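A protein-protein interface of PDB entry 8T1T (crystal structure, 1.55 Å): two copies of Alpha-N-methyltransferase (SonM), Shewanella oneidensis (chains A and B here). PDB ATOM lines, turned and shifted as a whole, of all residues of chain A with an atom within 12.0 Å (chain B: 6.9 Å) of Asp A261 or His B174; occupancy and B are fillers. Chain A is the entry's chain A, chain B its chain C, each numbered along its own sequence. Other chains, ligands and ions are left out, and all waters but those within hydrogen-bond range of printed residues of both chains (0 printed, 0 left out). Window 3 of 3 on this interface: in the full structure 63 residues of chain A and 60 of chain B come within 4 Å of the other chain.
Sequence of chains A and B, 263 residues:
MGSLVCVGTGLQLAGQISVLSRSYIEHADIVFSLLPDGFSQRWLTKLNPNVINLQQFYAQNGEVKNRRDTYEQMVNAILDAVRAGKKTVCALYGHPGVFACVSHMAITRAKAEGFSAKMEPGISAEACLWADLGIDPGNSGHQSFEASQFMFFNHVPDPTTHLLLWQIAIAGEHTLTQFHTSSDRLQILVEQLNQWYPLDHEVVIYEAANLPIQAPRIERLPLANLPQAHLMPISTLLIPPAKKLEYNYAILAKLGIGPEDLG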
ATOM      1  N   LEU A 245     -27.834  -6.441  -2.148  1.00  0.00           N
ATOM      2  CA  LEU A 245     -27.161  -5.954  -0.955  1.00  0.00           C
ATOM      3  C   LEU A 245     -27.086  -4.427  -0.977  1.00  0.00           C
ATOM      4  O   LEU A 245     -26.932  -3.820  -2.035  1.00  0.00           O
ATOM      5  CB  LEU A 245     -25.756  -6.562  -0.908  1.00  0.00           C
ATOM      6  CG  LEU A 245     -25.695  -8.064  -0.627  1.00  0.00           C
ATOM      7  CD1 LEU A 245     -24.288  -8.602  -0.846  1.00  0.00           C
ATOM      8  CD2 LEU A 245     -26.166  -8.367   0.786  1.00  0.00           C
ATOM      9  N   TYR A 247     -25.163  -1.074   1.149  1.00  0.00           N
ATOM     10  CA  TYR A 247     -24.000  -0.773   1.967  1.00  0.00           C
ATOM     11  C   TYR A 247     -24.428  -0.259   3.337  1.00  0.00           C
ATOM     12  O   TYR A 247     -25.377   0.512   3.459  1.00  0.00           O
ATOM     13  CB  TYR A 247     -23.113   0.270   1.284  1.00  0.00           C
ATOM     14  CG  TYR A 247     -22.538  -0.159  -0.042  1.00  0.00           C
ATOM     15  CD1 TYR A 247     -21.629  -1.201  -0.123  1.00  0.00           C
ATOM     16  CD2 TYR A 247     -22.912   0.467  -1.219  1.00  0.00           C
ATOM     17  CE1 TYR A 247     -21.096  -1.599  -1.337  1.00  0.00           C
ATOM     18  CE2 TYR A 247     -22.392   0.078  -2.442  1.00  0.00           C
ATOM     19  CZ  TYR A 247     -21.480  -0.960  -2.501  1.00  0.00           C
ATOM     20  OH  TYR A 247     -20.961  -1.352  -3.708  1.00  0.00           O
ATOM     21  N   ASN A 248     -23.681  -0.680   4.362  1.00  0.00           N
ATOM     22  CA  ASN A 248     -23.844  -0.184   5.714  1.00  0.00           C
ATOM     23  C   ASN A 248     -22.931   1.027   5.896  1.00  0.00           C
ATOM     24  O   ASN A 248     -21.841   0.905   6.450  1.00  0.00           O
ATOM     25  CB  ASN A 248     -23.504  -1.283   6.723  1.00  0.00           C
ATOM     26  CG  ASN A 248     -24.264  -1.165   8.024  1.00  0.00           C
ATOM     27  OD1 ASN A 248     -24.341  -0.087   8.610  1.00  0.00           O
ATOM     28  ND2 ASN A 248     -24.836  -2.272   8.472  1.00  0.00           N
ATOM     29  N   TYR A 249     -23.378   2.194   5.420  1.00  0.00           N
ATOM     30  CA  TYR A 249     -22.494   3.342   5.262  1.00  0.00           C
ATOM     31  C   TYR A 249     -21.911   3.792   6.601  1.00  0.00           C
ATOM     32  O   TYR A 249     -20.739   4.165   6.670  1.00  0.00           O
ATOM     33  CB  TYR A 249     -23.222   4.482   4.544  1.00  0.00           C
ATOM     34  CG  TYR A 249     -23.353   4.309   3.051  1.00  0.00           C
ATOM     35  CD1 TYR A 249     -22.245   4.359   2.224  1.00  0.00           C
ATOM     36  CD2 TYR A 249     -24.588   4.078   2.460  1.00  0.00           C
ATOM     37  CE1 TYR A 249     -22.354   4.205   0.853  1.00  0.00           C
ATOM     38  CE2 TYR A 249     -24.715   3.923   1.089  1.00  0.00           C
ATOM     39  CZ  TYR A 249     -23.595   3.983   0.283  1.00  0.00           C
ATOM     40  OH  TYR A 249     -23.702   3.830  -1.078  1.00  0.00           O
ATOM     41  N   ILE A 251     -21.176   2.081   9.198  1.00  0.00           N
ATOM     42  CA  ILE A 251     -20.157   1.144   9.645  1.00  0.00           C
ATOM     43  C   ILE A 251     -18.919   1.268   8.755  1.00  0.00           C
ATOM     44  O   ILE A 251     -17.797   1.289   9.255  1.00  0.00           O
ATOM     45  CB  ILE A 251     -20.714  -0.295   9.669  1.00  0.00           C
ATOM     46  CG1 ILE A 251     -21.949  -0.415  10.563  1.00  0.00           C
ATOM     47  CG2 ILE A 251     -19.635  -1.289  10.070  1.00  0.00           C
ATOM     48  CD1 ILE A 251     -21.689  -0.125  12.019  1.00  0.00           C
ATOM     49  N   LEU A 252     -19.131   1.362   7.437  1.00  0.00           N
ATOM     50  CA  LEU A 252     -18.033   1.491   6.492  1.00  0.00           C
ATOM     51  C   LEU A 252     -17.214   2.733   6.835  1.00  0.00           C
ATOM     52  O   LEU A 252     -15.986   2.684   6.847  1.00  0.00           O
ATOM     53  CB  LEU A 252     -18.587   1.556   5.066  1.00  0.00           C
ATOM     54  CG  LEU A 252     -19.292   0.292   4.571  1.00  0.00           C
ATOM     55  CD1 LEU A 252     -19.657   0.413   3.100  1.00  0.00           C
ATOM     56  CD2 LEU A 252     -18.427  -0.933   4.806  1.00  0.00           C
ATOM     57  N   ALA A 253     -17.910   3.834   7.141  1.00  0.00           N
ATOM     58  CA  ALA A 253     -17.258   5.089   7.474  1.00  0.00           C
ATOM     59  C   ALA A 253     -16.391   4.920   8.722  1.00  0.00           C
ATOM     60  O   ALA A 253     -15.283   5.452   8.782  1.00  0.00           O
ATOM     61  CB  ALA A 253     -18.290   6.172   7.663  1.00  0.00           C
ATOM     62  N   LYS A 254     -16.903   4.185   9.716  1.00  0.00           N
ATOM     63  CA  LYS A 254     -16.209   4.016  10.984  1.00  0.00           C
ATOM     64  C   LYS A 254     -14.999   3.102  10.807  1.00  0.00           C
ATOM     65  O   LYS A 254     -13.990   3.278  11.489  1.00  0.00           O
ATOM     66  CB  LYS A 254     -17.154   3.468  12.057  1.00  0.00           C
ATOM     67  CG  LYS A 254     -18.082   4.501  12.684  1.00  0.00           C
ATOM     68  CD  LYS A 254     -18.676   4.067  14.009  1.00  0.00           C
ATOM     69  CE  LYS A 254     -19.859   3.136  13.861  1.00  0.00           C
ATOM     70  NZ  LYS A 254     -21.048   3.846  13.335  1.00  0.00           N
ATOM     71  N   LEU A 255     -15.111   2.130   9.893  1.00  0.00           N
ATOM     72  CA  LEU A 255     -14.021   1.208   9.609  1.00  0.00           C
ATOM     73  C   LEU A 255     -13.020   1.870   8.663  1.00  0.00           C
ATOM     74  O   LEU A 255     -11.868   1.444   8.577  1.00  0.00           O
ATOM     75  CB  LEU A 255     -14.593  -0.070   8.987  1.00  0.00           C
ATOM     76  CG  LEU A 255     -15.412  -0.962   9.922  1.00  0.00           C
ATOM     77  CD1 LEU A 255     -16.080  -2.086   9.145  1.00  0.00           C
ATOM     78  CD2 LEU A 255     -14.542  -1.529  11.034  1.00  0.00           C
ATOM     79  N   GLY A 256     -13.478   2.897   7.940  1.00  0.00           N
ATOM     80  CA  GLY A 256     -12.621   3.658   7.046  1.00  0.00           C
ATOM     81  C   GLY A 256     -12.458   2.996   5.680  1.00  0.00           C
ATOM     82  O   GLY A 256     -11.398   3.088   5.068  1.00  0.00           O
ATOM     83  N   ILE A 257     -13.521   2.339   5.202  1.00  0.00           N
ATOM     84  CA  ILE A 257     -13.513   1.712   3.890  1.00  0.00           C
ATOM     85  C   ILE A 257     -14.759   2.167   3.134  1.00  0.00           C
ATOM     86  O   ILE A 257     -15.613   2.845   3.701  1.00  0.00           O
ATOM     87  CB  ILE A 257     -13.424   0.177   4.014  1.00  0.00           C
ATOM     88  CG1 ILE A 257     -14.740  -0.441   4.490  1.00  0.00           C
ATOM     89  CG2 ILE A 257     -12.259  -0.231   4.904  1.00  0.00           C
ATOM     90  CD1 ILE A 257     -15.824  -0.446   3.437  1.00  0.00           C
ATOM     91  N   GLY A 258     -14.850   1.797   1.850  1.00  0.00           N
ATOM     92  CA  GLY A 258     -15.959   2.226   1.013  1.00  0.00           C
ATOM     93  C   GLY A 258     -16.330   1.191  -0.046  1.00  0.00           C
ATOM     94  O   GLY A 258     -15.662   0.169  -0.186  1.00  0.00           O
ATOM     95  N   PRO A 259     -17.413   1.429  -0.819  1.00  0.00           N
ATOM     96  CA  PRO A 259     -17.834   0.505  -1.872  1.00  0.00           C
ATOM     97  C   PRO A 259     -16.697   0.122  -2.817  1.00  0.00           C
ATOM     98  O   PRO A 259     -16.602  -1.025  -3.247  1.00  0.00           O
ATOM     99  CB  PRO A 259     -18.920   1.290  -2.625  1.00  0.00           C
ATOM    100  CG  PRO A 259     -19.482   2.238  -1.582  1.00  0.00           C
ATOM    101  CD  PRO A 259     -18.300   2.597  -0.704  1.00  0.00           C
ATOM    102  N   GLU A 260     -15.838   1.100  -3.122  1.00  0.00           N
ATOM    103  CA  GLU A 260     -14.737   0.912  -4.052  1.00  0.00           C
ATOM    104  C   GLU A 260     -14.107  -0.464  -3.844  1.00  0.00           C
ATOM    105  O   GLU A 260     -13.952  -1.230  -4.794  1.00  0.00           O
ATOM    106  CB  GLU A 260     -13.676   2.001  -3.870  1.00  0.00           C
ATOM    107  CG  GLU A 260     -14.199   3.415  -4.065  1.00  0.00           C
ATOM    108  CD  GLU A 260     -14.876   4.029  -2.850  1.00  0.00           C
ATOM    109  OE1 GLU A 260     -15.885   3.466  -2.387  1.00  0.00           O
ATOM    110  OE2 GLU A 260     -14.388   5.073  -2.369  1.00  0.00           O
ATOM    111  N   ASP A 261     -13.751  -0.765  -2.589  1.00  0.00           N
ATOM    112  CA  ASP A 261     -12.938  -1.928  -2.278  1.00  0.00           C
ATOM    113  C   ASP A 261     -13.800  -3.026  -1.656  1.00  0.00           C
ATOM    114  O   ASP A 261     -13.363  -3.719  -0.739  1.00  0.00           O
ATOM    115  CB  ASP A 261     -11.766  -1.531  -1.375  1.00  0.00           C
ATOM    116  CG  ASP A 261     -12.170  -0.736  -0.145  1.00  0.00           C
ATOM    117  OD1 ASP A 261     -12.867  -1.306   0.718  1.00  0.00           O
ATOM    118  OD2 ASP A 261     -11.790   0.451  -0.062  1.00  0.00           O
ATOM    119  N   LEU A 262     -15.021  -3.191  -2.180  1.00  0.00           N
ATOM    120  CA  LEU A 262     -15.915  -4.257  -1.754  1.00  0.00           C
ATOM    121  C   LEU A 262     -16.383  -5.051  -2.969  1.00  0.00           C
ATOM    122  O   LEU A 262     -15.569  -5.597  -3.711  1.00  0.00           O
ATOM    123  CB  LEU A 262     -17.109  -3.655  -1.003  1.00  0.00           C
ATOM    124  CG  LEU A 262     -16.943  -3.503   0.507  1.00  0.00           C
ATOM    125  CD1 LEU A 262     -15.891  -2.459   0.842  1.00  0.00           C
ATOM    126  CD2 LEU A 262     -18.270  -3.145   1.159  1.00  0.00           C
ATOM    127  N   GLY A 263     -17.706  -5.110  -3.154  1.00  0.00           N
ATOM    128  CA  GLY A 263     -18.310  -5.879  -4.228  1.00  0.00           C
ATOM    129  C   GLY A 263     -19.672  -6.423  -3.828  1.00  0.00           C
ATOM    130  O   GLY A 263     -19.740  -7.640  -3.560  1.00  0.00           O
ATOM    131  OXT GLY A 263     -20.621  -5.612  -3.792  1.00  0.00           O
ATOM    132  N   ASN B  66      -2.437 -10.172  -2.001  1.00  0.00           N
ATOM    133  CA  ASN B  66      -3.853 -10.183  -1.678  1.00  0.00           C
ATOM    134  C   ASN B  66      -4.311 -11.636  -1.592  1.00  0.00           C
ATOM    135  O   ASN B  66      -3.925 -12.459  -2.419  1.00  0.00           O
ATOM    136  CB  ASN B  66      -4.670  -9.391  -2.702  1.00  0.00           C
ATOM    137  CG  ASN B  66      -6.131  -9.259  -2.325  1.00  0.00           C
ATOM    138  OD1 ASN B  66      -6.537  -9.661  -1.237  1.00  0.00           O
ATOM    139  ND2 ASN B  66      -6.928  -8.689  -3.214  1.00  0.00           N
ATOM    140  N   ARG B  68      -6.711 -12.867  -2.441  1.00  0.00           N
ATOM    141  CA  ARG B  68      -7.363 -13.216  -3.692  1.00  0.00           C
ATOM    142  C   ARG B  68      -6.334 -13.818  -4.648  1.00  0.00           C
ATOM    143  O   ARG B  68      -6.658 -14.706  -5.435  1.00  0.00           O
ATOM    144  CB  ARG B  68      -8.017 -11.987  -4.330  1.00  0.00           C
ATOM    145  CG  ARG B  68      -9.321 -11.555  -3.676  1.00  0.00           C
ATOM    146  CD  ARG B  68     -10.011 -10.464  -4.472  1.00  0.00           C
ATOM    147  NE  ARG B  68     -11.376 -10.219  -4.028  1.00  0.00           N
ATOM    148  CZ  ARG B  68     -12.219  -9.379  -4.618  1.00  0.00           C
ATOM    149  NH1 ARG B  68     -11.831  -8.686  -5.674  1.00  0.00           N
ATOM    150  NH2 ARG B  68     -13.447  -9.233  -4.150  1.00  0.00           N
ATOM    151  N   SER B 148     -17.661 -10.127   8.556  1.00  0.00           N
ATOM    152  CA  SER B 148     -17.372  -8.915   7.803  1.00  0.00           C
ATOM    153  C   SER B 148     -18.552  -8.530   6.909  1.00  0.00           C
ATOM    154  O   SER B 148     -18.863  -7.348   6.778  1.00  0.00           O
ATOM    155  CB  SER B 148     -16.106  -9.058   7.000  1.00  0.00           C
ATOM    156  OG  SER B 148     -14.961  -8.977   7.840  1.00  0.00           O
ATOM    157  N   PHE B 152     -20.570  -5.019   6.735  1.00  0.00           N
ATOM    158  CA  PHE B 152     -20.426  -4.199   5.539  1.00  0.00           C
ATOM    159  C   PHE B 152     -21.780  -3.907   4.896  1.00  0.00           C
ATOM    160  O   PHE B 152     -21.959  -2.862   4.272  1.00  0.00           O
ATOM    161  CB  PHE B 152     -19.548  -4.904   4.502  1.00  0.00           C
ATOM    162  CG  PHE B 152     -18.096  -5.069   4.879  1.00  0.00           C
ATOM    163  CD1 PHE B 152     -17.546  -4.361   5.934  1.00  0.00           C
ATOM    164  CD2 PHE B 152     -17.286  -5.955   4.183  1.00  0.00           C
ATOM    165  CE1 PHE B 152     -16.210  -4.519   6.274  1.00  0.00           C
ATOM    166  CE2 PHE B 152     -15.952  -6.113   4.526  1.00  0.00           C
ATOM    167  CZ  PHE B 152     -15.418  -5.392   5.568  1.00  0.00           C
ATOM    168  N   ILE B 170     -11.404 -11.700  12.074  1.00  0.00           N
ATOM    169  CA  ILE B 170     -11.058 -10.686  11.089  1.00  0.00           C
ATOM    170  C   ILE B 170     -12.284  -9.840  10.751  1.00  0.00           C
ATOM    171  O   ILE B 170     -12.325  -9.213   9.696  1.00  0.00           O
ATOM    172  CB  ILE B 170     -10.454 -11.324   9.821  1.00  0.00           C
ATOM    173  CG1 ILE B 170     -11.431 -12.290   9.144  1.00  0.00           C
ATOM    174  CG2 ILE B 170      -9.122 -11.988  10.132  1.00  0.00           C
ATOM    175  CD1 ILE B 170     -10.953 -12.817   7.812  1.00  0.00           C
ATOM    176  N   ALA B 171     -13.263  -9.803  11.662  1.00  0.00           N
ATOM    177  CA  ALA B 171     -14.470  -9.015  11.459  1.00  0.00           C
ATOM    178  C   ALA B 171     -14.109  -7.562  11.145  1.00  0.00           C
ATOM    179  O   ALA B 171     -13.503  -6.870  11.960  1.00  0.00           O
ATOM    180  CB  ALA B 171     -15.358  -9.105  12.678  1.00  0.00           C
ATOM    181  N   GLY B 172     -14.486  -7.111   9.944  1.00  0.00           N
ATOM    182  CA  GLY B 172     -14.372  -5.710   9.573  1.00  0.00           C
ATOM    183  C   GLY B 172     -13.037  -5.377   8.909  1.00  0.00           C
ATOM    184  O   GLY B 172     -12.807  -4.231   8.529  1.00  0.00           O
ATOM    185  N   GLU B 173     -12.167  -6.383   8.765  1.00  0.00           N
ATOM    186  CA  GLU B 173     -10.841  -6.173   8.205  1.00  0.00           C
ATOM    187  C   GLU B 173     -10.918  -6.060   6.684  1.00  0.00           C
ATOM    188  O   GLU B 173     -11.747  -6.707   6.048  1.00  0.00           O
ATOM    189  CB  GLU B 173      -9.900  -7.321   8.573  1.00  0.00           C
ATOM    190  CG  GLU B 173      -9.245  -7.175   9.933  1.00  0.00           C
ATOM    191  CD  GLU B 173      -8.248  -8.277  10.247  1.00  0.00           C
ATOM    192  OE1 GLU B 173      -8.242  -8.765  11.395  1.00  0.00           O
ATOM    193  OE2 GLU B 173      -7.493  -8.662   9.332  1.00  0.00           O
ATOM    194  N   HIS B 174     -10.034  -5.230   6.120  1.00  0.00           N
ATOM    195  CA  HIS B 174      -9.822  -5.183   4.683  1.00  0.00           C
ATOM    196  C   HIS B 174      -8.494  -4.487   4.395  1.00  0.00           C
ATOM    197  O   HIS B 174      -8.296  -3.334   4.774  1.00  0.00           O
ATOM    198  CB  HIS B 174     -10.990  -4.492   3.970  1.00  0.00           C
ATOM    199  CG  HIS B 174     -11.015  -4.760   2.502  1.00  0.00           C
ATOM    200  ND1 HIS B 174     -10.749  -3.802   1.548  1.00  0.00           N
ATOM    201  CD2 HIS B 174     -11.248  -5.896   1.829  1.00  0.00           C
ATOM    202  CE1 HIS B 174     -10.834  -4.349   0.343  1.00  0.00           C
ATOM    203  NE2 HIS B 174     -11.138  -5.620   0.490  1.00  0.00           N
ATOM    204  N   THR B 175      -7.589  -5.218   3.734  1.00  0.00           N
ATOM    205  CA  THR B 175      -6.310  -4.692   3.284  1.00  0.00           C
ATOM    206  C   THR B 175      -6.004  -3.353   3.954  1.00  0.00           C
ATOM    207  O   THR B 175      -5.375  -3.315   5.011  1.00  0.00           O
ATOM    208  CB  THR B 175      -6.283  -4.576   1.754  1.00  0.00           C
ATOM    209  OG1 THR B 175      -7.358  -3.726   1.351  1.00  0.00           O
ATOM    210  CG2 THR B 175      -6.412  -5.915   1.059  1.00  0.00           C
ATOM    211  N   LEU B 176      -6.450  -2.259   3.323  1.00  0.00           N
ATOM    212  CA  LEU B 176      -6.016  -0.917   3.685  1.00  0.00           C
ATOM    213  C   LEU B 176      -6.759  -0.433   4.928  1.00  0.00           C
ATOM    214  O   LEU B 176      -7.939  -0.738   5.113  1.00  0.00           O
ATOM    215  CB  LEU B 176      -6.259   0.023   2.498  1.00  0.00           C
ATOM    216  CG  LEU B 176      -5.543  -0.353   1.201  1.00  0.00           C
ATOM    217  CD1 LEU B 176      -4.211  -1.035   1.491  1.00  0.00           C
ATOM    218  CD2 LEU B 176      -6.418  -1.240   0.324  1.00  0.00           C
ATOM    219  N   THR B 177      -6.048   0.342   5.760  1.00  0.00           N
ATOM    220  CA  THR B 177      -6.586   0.860   7.008  1.00  0.00           C
ATOM    221  C   THR B 177      -6.652  -0.272   8.029  1.00  0.00           C
ATOM    222  O   THR B 177      -7.638  -1.003   8.090  1.00  0.00           O
ATOM    223  CB  THR B 177      -7.954   1.525   6.793  1.00  0.00           C
ATOM    224  OG1 THR B 177      -8.887   0.534   6.362  1.00  0.00           O
ATOM    225  CG2 THR B 177      -7.906   2.653   5.785  1.00  0.00           C
ATOM    226  N   GLN B 178      -5.589  -0.402   8.832  1.00  0.00           N
ATOM    227  CA  GLN B 178      -5.460  -1.511   9.762  1.00  0.00           C
ATOM    228  C   GLN B 178      -6.017  -1.116  11.127  1.00  0.00           C
ATOM    229  O   GLN B 178      -5.386  -0.366  11.872  1.00  0.00           O
ATOM    230  CB  GLN B 178      -3.999  -1.945   9.905  1.00  0.00           C
ATOM    231  CG  GLN B 178      -3.316  -2.273   8.585  1.00  0.00           C
ATOM    232  CD  GLN B 178      -2.622  -1.077   7.976  1.00  0.00           C
ATOM    233  OE1 GLN B 178      -3.248  -0.076   7.634  1.00  0.00           O
ATOM    234  NE2 GLN B 178      -1.311  -1.178   7.834  1.00  0.00           N
ATOM    235  N   HIS B 180      -6.254  -3.489  13.143  1.00  0.00           N
ATOM    236  CA  HIS B 180      -5.850  -4.791  13.644  1.00  0.00           C
ATOM    237  C   HIS B 180      -5.908  -4.764  15.168  1.00  0.00           C
ATOM    238  O   HIS B 180      -5.525  -5.729  15.829  1.00  0.00           O
ATOM    239  CB  HIS B 180      -4.511  -5.204  13.026  1.00  0.00           C
ATOM    240  CG  HIS B 180      -4.661  -5.607  11.598  1.00  0.00           C
ATOM    241  ND1 HIS B 180      -4.256  -4.821  10.541  1.00  0.00           N
ATOM    242  CD2 HIS B 180      -5.221  -6.697  11.056  1.00  0.00           C
ATOM    243  CE1 HIS B 180      -4.544  -5.437   9.403  1.00  0.00           C
ATOM    244  NE2 HIS B 180      -5.128  -6.580   9.692  1.00  0.00           N
ATOM    245  N   ARG B 185     -12.508  -2.955  16.077  1.00  0.00           N
ATOM    246  CA  ARG B 185     -13.445  -3.505  15.107  1.00  0.00           C
ATOM    247  C   ARG B 185     -14.592  -4.218  15.818  1.00  0.00           C
ATOM    248  O   ARG B 185     -15.735  -4.147  15.370  1.00  0.00           O
ATOM    249  CB  ARG B 185     -12.740  -4.487  14.165  1.00  0.00           C
ATOM    250  CG  ARG B 185     -11.883  -3.836  13.088  1.00  0.00           C
ATOM    251  CD  ARG B 185     -11.062  -4.860  12.323  1.00  0.00           C
ATOM    252  NE  ARG B 185      -9.989  -5.425  13.129  1.00  0.00           N
ATOM    253  CZ  ARG B 185      -9.928  -6.686  13.548  1.00  0.00           C
ATOM    254  NH1 ARG B 185     -10.900  -7.536  13.269  1.00  0.00           N
ATOM    255  NH2 ARG B 185      -8.892  -7.089  14.264  1.00  0.00           N
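No position is printed for both chains.
Of the 10 pairs that touch across the chains among the printed residues, none has its exchanged pair printed and touching as well.
O of Phe B152 sits at hydrogen-bond distance from N of Asn A248 (2.8 Å).
O of Asp A261 lies close to NE2 of His B174 (3.2 Å).
Hydrophobic or aromatic side chains of chain B that line the printed part of chain A: Phe B152 and His B174.
Asp A261 touches just one residue of chain B: His B174.
His B174 touches just one residue of chain A: Asp A261.
Of chain A, only Leu A255 (3.96 Å) comes within 4 Å of Gly B172.
No residue of chain A comes within 4 Å of Glu B173.
No residue of chain A comes within 4 Å of Leu B176.
Printed residues of chain A within 4 Å of Thr B177: Leu A255, Gly A256 and Ile A257.
Of the printed residues of chain B, Leu A262 touches Phe B152 (3.99 Å).
Printed residues of chain A within 4 Å of Phe B152: Tyr A247 (3.7 Å), Asn A248 (2.8 Å), Leu A252 (3.7 Å), Leu A255 (3.8 Å) and Leu A262 (3.99 Å).
Of the printed residues of chain B, Tyr A247 touches Phe B152 (3.7 Å).
Of the printed residues of chain B, Ile A257 touches Thr B177 (3.8 Å).
Of the printed residues of chain B, Asn A248 touches Phe B152.
Arg B185 touches none of the printed residues of chain A.
The nearest printed residue of chain B that does not touch Asp A261 is Leu B176 (5.6 Å).
The nearest residue of chain A that does not touch His B174 is Ile A257 (4.5 Å).
Among the printed residues, merely in contact across the chains: Gly A256 with Thr B177, Tyr A247 with Phe B152, Leu A252 with Phe B152, Ile A257 with Thr B177, Leu A255 with Phe B152, Leu A255 with Thr B177, Leu A255 with Gly B172 and Leu A262 with Phe B152.
N of Ile A257 lies within hydrogen-bond range of O of Leu A252 (3.0 Å).
OG of Ser B148 lies within hydrogen-bond range of N of Gly B172 (2.9 Å).
ND1 of His B174 lies close to OG1 of Thr B175 (3.4 Å).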
